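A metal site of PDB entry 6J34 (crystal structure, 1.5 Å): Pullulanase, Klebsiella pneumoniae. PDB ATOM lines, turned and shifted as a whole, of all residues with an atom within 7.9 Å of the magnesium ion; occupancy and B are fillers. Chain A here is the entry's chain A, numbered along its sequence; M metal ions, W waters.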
ATOM      1  N   SER A 929      23.220  24.554  13.762  1.00  0.00           N
ATOM      2  CA  SER A 929      24.228  23.500  13.928  1.00  0.00           C
ATOM      3  C   SER A 929      25.594  24.091  14.210  1.00  0.00           C
ATOM      4  O   SER A 929      26.014  25.042  13.524  1.00  0.00           O
ATOM      5  CB  SER A 929      24.328  22.614  12.674  1.00  0.00           C
ATOM      6  OG  SER A 929      25.389  21.679  12.791  1.00  0.00           O
ATOM      7  N   LEU A 931      28.217  22.799  13.263  1.00  0.00           N
ATOM      8  CA  LEU A 931      29.081  22.476  12.127  1.00  0.00           C
ATOM      9  C   LEU A 931      29.312  23.691  11.216  1.00  0.00           C
ATOM     10  O   LEU A 931      30.338  23.748  10.529  1.00  0.00           O
ATOM     11  CB  LEU A 931      28.491  21.318  11.333  1.00  0.00           C
ATOM     12  CG  LEU A 931      28.473  19.980  12.073  1.00  0.00           C
ATOM     13  CD1 LEU A 931      27.750  18.940  11.249  1.00  0.00           C
ATOM     14  CD2 LEU A 931      29.879  19.524  12.373  1.00  0.00           C
ATOM     15  N   ARG A 943      37.463  19.007   8.588  1.00  0.00           N
ATOM     16  CA  ARG A 943      36.049  18.722   8.351  1.00  0.00           C
ATOM     17  C   ARG A 943      35.465  19.281   7.048  1.00  0.00           C
ATOM     18  O   ARG A 943      34.483  18.734   6.556  1.00  0.00           O
ATOM     19  CB  ARG A 943      35.198  19.232   9.537  1.00  0.00           C
ATOM     20  CG  ARG A 943      35.512  18.489  10.842  1.00  0.00           C
ATOM     21  CD  ARG A 943      34.694  19.038  12.006  1.00  0.00           C
ATOM     22  NE  ARG A 943      34.963  18.343  13.283  1.00  0.00           N
ATOM     23  CZ  ARG A 943      34.114  17.508  13.881  1.00  0.00           C
ATOM     24  NH1 ARG A 943      32.934  17.235  13.319  1.00  0.00           N
ATOM     25  NH2 ARG A 943      34.445  16.954  15.045  1.00  0.00           N
ATOM     26  N   ASP A 963      32.067  17.669   7.648  1.00  0.00           N
ATOM     27  CA  ASP A 963      32.052  16.318   8.186  1.00  0.00           C
ATOM     28  C   ASP A 963      31.753  16.321   9.692  1.00  0.00           C
ATOM     29  O   ASP A 963      32.336  17.107  10.451  1.00  0.00           O
ATOM     30  CB  ASP A 963      33.427  15.677   7.945  1.00  0.00           C
ATOM     31  CG  ASP A 963      33.437  14.205   8.221  1.00  0.00           C
ATOM     32  OD1 ASP A 963      32.353  13.575   8.240  1.00  0.00           O
ATOM     33  OD2 ASP A 963      34.548  13.671   8.415  1.00  0.00           O
ATOM     34  N   ASP A 964      30.833  15.446  10.115  1.00  0.00           N
ATOM     35  CA  ASP A 964      30.652  15.123  11.532  1.00  0.00           C
ATOM     36  C   ASP A 964      30.852  13.633  11.801  1.00  0.00           C
ATOM     37  O   ASP A 964      30.488  13.146  12.882  1.00  0.00           O
ATOM     38  CB  ASP A 964      29.286  15.578  12.059  1.00  0.00           C
ATOM     39  CG  ASP A 964      29.300  15.881  13.572  1.00  0.00           C
ATOM     40  OD1 ASP A 964      30.329  16.396  14.070  1.00  0.00           O
ATOM     41  OD2 ASP A 964      28.286  15.602  14.256  1.00  0.00           O
ATOM     42  N   GLY A 965      31.441  12.909  10.843  1.00  0.00           N
ATOM     43  CA  GLY A 965      31.613  11.486  10.956  1.00  0.00           C
ATOM     44  C   GLY A 965      32.887  11.081  11.687  1.00  0.00           C
ATOM     45  O   GLY A 965      33.664  11.906  12.174  1.00  0.00           O
ATOM     46  N   ALA A 970      35.067  13.780  17.213  1.00  0.00           N
ATOM     47  CA  ALA A 970      33.809  13.650  17.917  1.00  0.00           C
ATOM     48  C   ALA A 970      32.654  14.191  17.093  1.00  0.00           C
ATOM     49  O   ALA A 970      32.823  15.070  16.239  1.00  0.00           O
ATOM     50  CB  ALA A 970      33.868  14.408  19.248  1.00  0.00           C
ATOM     51  N   SER A 971      31.465  13.651  17.336  1.00  0.00           N
ATOM     52  CA  SER A 971      30.253  14.248  16.777  1.00  0.00           C
ATOM     53  C   SER A 971      29.959  15.530  17.559  1.00  0.00           C
ATOM     54  O   SER A 971      29.803  15.487  18.780  1.00  0.00           O
ATOM     55  CB  SER A 971      29.090  13.265  16.909  1.00  0.00           C
ATOM     56  OG  SER A 971      27.837  13.866  16.603  1.00  0.00           O
ATOM     57  N   LEU A 972      29.953  16.661  16.850  1.00  0.00           N
ATOM     58  CA  LEU A 972      29.620  17.941  17.453  1.00  0.00           C
ATOM     59  C   LEU A 972      28.123  18.211  17.431  1.00  0.00           C
ATOM     60  O   LEU A 972      27.635  19.078  18.168  1.00  0.00           O
ATOM     61  CB  LEU A 972      30.338  19.074  16.730  1.00  0.00           C
ATOM     62  CG  LEU A 972      31.872  18.980  16.646  1.00  0.00           C
ATOM     63  CD1 LEU A 972      32.427  20.068  15.746  1.00  0.00           C
ATOM     64  CD2 LEU A 972      32.495  19.051  18.035  1.00  0.00           C
ATOM     65  N   ASP A 973      27.382  17.475  16.600  1.00  0.00           N
ATOM     66  CA  ASP A 973      25.960  17.664  16.429  1.00  0.00           C
ATOM     67  C   ASP A 973      25.321  16.290  16.508  1.00  0.00           C
ATOM     68  O   ASP A 973      25.606  15.428  15.662  1.00  0.00           O
ATOM     69  CB  ASP A 973      25.698  18.339  15.077  1.00  0.00           C
ATOM     70  CG  ASP A 973      24.258  18.755  14.868  1.00  0.00           C
ATOM     71  OD1 ASP A 973      23.343  18.170  15.486  1.00  0.00           O
ATOM     72  OD2 ASP A 973      24.033  19.671  14.046  1.00  0.00           O
ATOM     73  N   SER A 974      24.482  16.069  17.520  1.00  0.00           N
ATOM     74  CA  SER A 974      23.896  14.751  17.705  1.00  0.00           C
ATOM     75  C   SER A 974      22.862  14.411  16.650  1.00  0.00           C
ATOM     76  O   SER A 974      22.491  13.229  16.513  1.00  0.00           O
ATOM     77  CB  SER A 974      23.235  14.637  19.081  1.00  0.00           C
ATOM     78  OG  SER A 974      22.145  15.533  19.188  1.00  0.00           O
ATOM     79  N   ARG A 975      22.378  15.398  15.905  1.00  0.00           N
ATOM     80  CA  ARG A 975      21.336  15.139  14.925  1.00  0.00           C
ATOM     81  C   ARG A 975      21.865  14.751  13.567  1.00  0.00           C
ATOM     82  O   ARG A 975      21.126  14.149  12.773  1.00  0.00           O
ATOM     83  CB  ARG A 975      20.425  16.365  14.787  1.00  0.00           C
ATOM     84  CG  ARG A 975      19.718  16.740  16.077  1.00  0.00           C
ATOM     85  CD  ARG A 975      18.617  17.774  15.828  1.00  0.00           C
ATOM     86  NE  ARG A 975      17.980  18.205  17.069  1.00  0.00           N
ATOM     87  CZ  ARG A 975      16.942  19.032  17.130  1.00  0.00           C
ATOM     88  NH1 ARG A 975      16.414  19.531  16.006  1.00  0.00           N
ATOM     89  NH2 ARG A 975      16.420  19.371  18.302  1.00  0.00           N
ATOM     90  N   VAL A 976      23.117  15.079  13.235  1.00  0.00           N
ATOM     91  CA  VAL A 976      23.652  14.850  11.897  1.00  0.00           C
ATOM     92  C   VAL A 976      25.062  14.287  11.953  1.00  0.00           C
ATOM     93  O   VAL A 976      25.829  14.548  12.886  1.00  0.00           O
ATOM     94  CB  VAL A 976      23.625  16.129  11.022  1.00  0.00           C
ATOM     95  CG1 VAL A 976      22.230  16.683  10.909  1.00  0.00           C
ATOM     96  CG2 VAL A 976      24.588  17.184  11.586  1.00  0.00           C
ATOM     97  N   ASP A 977      25.407  13.518  10.908  1.00  0.00           N
ATOM     98  CA  ASP A 977      26.761  13.063  10.653  1.00  0.00           C
ATOM     99  C   ASP A 977      27.499  13.910   9.625  1.00  0.00           C
ATOM    100  O   ASP A 977      28.670  13.659   9.346  1.00  0.00           O
ATOM    101  CB  ASP A 977      26.746  11.616  10.120  1.00  0.00           C
ATOM    102  CG  ASP A 977      26.475  10.577  11.201  1.00  0.00           C
ATOM    103  OD1 ASP A 977      26.919  10.752  12.362  1.00  0.00           O
ATOM    104  OD2 ASP A 977      25.830   9.564  10.858  1.00  0.00           O
ATOM    105  N   GLY A 978      26.827  14.901   9.044  1.00  0.00           N
ATOM    106  CA  GLY A 978      27.450  15.732   8.031  1.00  0.00           C
ATOM    107  C   GLY A 978      26.442  16.680   7.419  1.00  0.00           C
ATOM    108  O   GLY A 978      25.238  16.438   7.493  1.00  0.00           O
ATOM    109  N   LEU A1038      23.148  14.467   6.596  1.00  0.00           N
ATOM    110  CA  LEU A1038      23.141  13.043   6.826  1.00  0.00           C
ATOM    111  C   LEU A1038      22.556  12.809   8.208  1.00  0.00           C
ATOM    112  O   LEU A1038      23.183  13.198   9.198  1.00  0.00           O
ATOM    113  CB  LEU A1038      24.561  12.486   6.755  1.00  0.00           C
ATOM    114  CG  LEU A1038      25.273  12.530   5.402  1.00  0.00           C
ATOM    115  CD1 LEU A1038      26.675  11.987   5.533  1.00  0.00           C
ATOM    116  CD2 LEU A1038      24.499  11.773   4.334  1.00  0.00           C
ATOM    117  N   PRO A1039      21.379  12.204   8.334  1.00  0.00           N
ATOM    118  CA  PRO A1039      20.798  12.003   9.670  1.00  0.00           C
ATOM    119  C   PRO A1039      21.652  11.051  10.487  1.00  0.00           C
ATOM    120  O   PRO A1039      22.130  10.028   9.995  1.00  0.00           O
ATOM    121  CB  PRO A1039      19.429  11.371   9.376  1.00  0.00           C
ATOM    122  CG  PRO A1039      19.302  11.264   7.893  1.00  0.00           C
ATOM    123  CD  PRO A1039      20.620  11.540   7.256  1.00  0.00           C
ATOM    124  N   GLN A1040      21.829  11.379  11.767  1.00  0.00           N
ATOM    125  CA  GLN A1040      22.641  10.548  12.660  1.00  0.00           C
ATOM    126  C   GLN A1040      21.768   9.505  13.323  1.00  0.00           C
ATOM    127  O   GLN A1040      20.668   9.813  13.807  1.00  0.00           O
ATOM    128  CB  GLN A1040      23.331  11.406  13.717  1.00  0.00           C
ATOM    129  CG  GLN A1040      24.295  10.616  14.608  1.00  0.00           C
ATOM    130  CD  GLN A1040      25.258  11.529  15.331  1.00  0.00           C
ATOM    131  OE1 GLN A1040      25.481  12.667  14.898  1.00  0.00           O
ATOM    132  NE2 GLN A1040      25.831  11.052  16.422  1.00  0.00           N
ATOM    133  N   GLY A1041      22.248   8.268  13.342  1.00  0.00           N
ATOM    134  CA  GLY A1041      21.528   7.173  13.944  1.00  0.00           C
ATOM    135  C   GLY A1041      22.062   6.817  15.313  1.00  0.00           C
ATOM    136  O   GLY A1041      22.481   7.689  16.087  1.00  0.00           O
ATOM    137  N   SER A1043      24.732   5.387  16.426  1.00  0.00           N
ATOM    138  CA  SER A1043      26.104   5.770  16.653  1.00  0.00           C
ATOM    139  C   SER A1043      26.581   6.719  15.593  1.00  0.00           C
ATOM    140  O   SER A1043      26.012   6.798  14.536  1.00  0.00           O
ATOM    141  CB  SER A1043      27.014   4.560  16.531  1.00  0.00           C
ATOM    142  OG  SER A1043      26.601   3.557  17.390  1.00  0.00           O
ATOM    143  N   GLN A1044      27.645   7.448  15.882  1.00  0.00           N
ATOM    144  CA  GLN A1044      28.262   8.291  14.869  1.00  0.00           C
ATOM    145  C   GLN A1044      28.552   7.481  13.614  1.00  0.00           C
ATOM    146  O   GLN A1044      29.031   6.346  13.681  1.00  0.00           O
ATOM    147  CB  GLN A1044      29.564   8.858  15.426  1.00  0.00           C
ATOM    148  CG  GLN A1044      30.306   9.785  14.493  1.00  0.00           C
ATOM    149  CD  GLN A1044      31.573  10.296  15.129  1.00  0.00           C
ATOM    150  OE1 GLN A1044      32.192   9.607  15.945  1.00  0.00           O
ATOM    151  NE2 GLN A1044      31.971  11.509  14.764  1.00  0.00           N
ATOM    152  N   GLY A1045      28.229   8.063  12.462  1.00  0.00           N
ATOM    153  CA  GLY A1045      28.359   7.388  11.189  1.00  0.00           C
ATOM    154  C   GLY A1045      29.598   7.799  10.408  1.00  0.00           C
ATOM    155  O   GLY A1045      30.503   8.458  10.923  1.00  0.00           O
HETATM  156 MG    MG M   1      26.846  14.226  14.659  1.00  0.00          MG
HETATM  157  O   HOH W   1      27.982  12.720  13.873  1.00  0.00           O
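The side-chain amide nitrogen of Gln 1044 sits at hydrogen-bond distance from the backbone carbonyl oxygen of Asp 964, at 2.9 Å. The backbone NH (N) of Arg 975 sits at hydrogen-bond distance from the side-chain carboxylate (OD1) of Asp 973 (3.0 Å). The backbone carbonyl oxygen of Ser 974 sits close to the side-chain amide oxygen of Gln 1040 (3.4 Å). The side-chain amide oxygen (OE1) of Gln 1040 sits close to the side-chain carboxylate (OD1) of Asp 977, at 3.5 Å. The side-chain carboxylate (OD1) of Asp 964 is in hydrogen-bond range of the backbone NH (N) of Leu 972 (2.8 Å). N of Asp 964 sits at hydrogen-bond distance from O of Asp 977 (2.9 Å). The backbone NH of Gln 1040 is in hydrogen-bond range of the backbone carbonyl oxygen of Arg 975. The side-chain amide nitrogen (NE2) of Gln 1044 sits close to the backbone NH (N) of Ser 971.
Water W1 lies within hydrogen-bond range of OD1 of Asp 977 (2.7 Å) and O of Asp 964 (2.7 Å).
Of the 22 residues printed, 5 come within 4 Å of the magnesium ion. Along chain A the residues within 4 Å of the magnesium ion span positions 964 to 1040. The nearest printed residue that does not touch the magnesium ion is Asp 977 (4.1 Å).
The magnesium ion is bound by O of Asp 973, 2.0 Å away. OD2 of Asp 964 binds the magnesium ion (2.0 Å). Water W1 is bound to the magnesium ion. The backbone carbonyl oxygen (O) of Val 976 is bound to the magnesium ion, 2.1 Å away. The side-chain amide oxygen (OE1) of Gln 1040 is bound to the magnesium ion (2.1 Å). The magnesium ion is bound by the side-chain hydroxyl (OG) of Ser 971 (2.2 Å).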
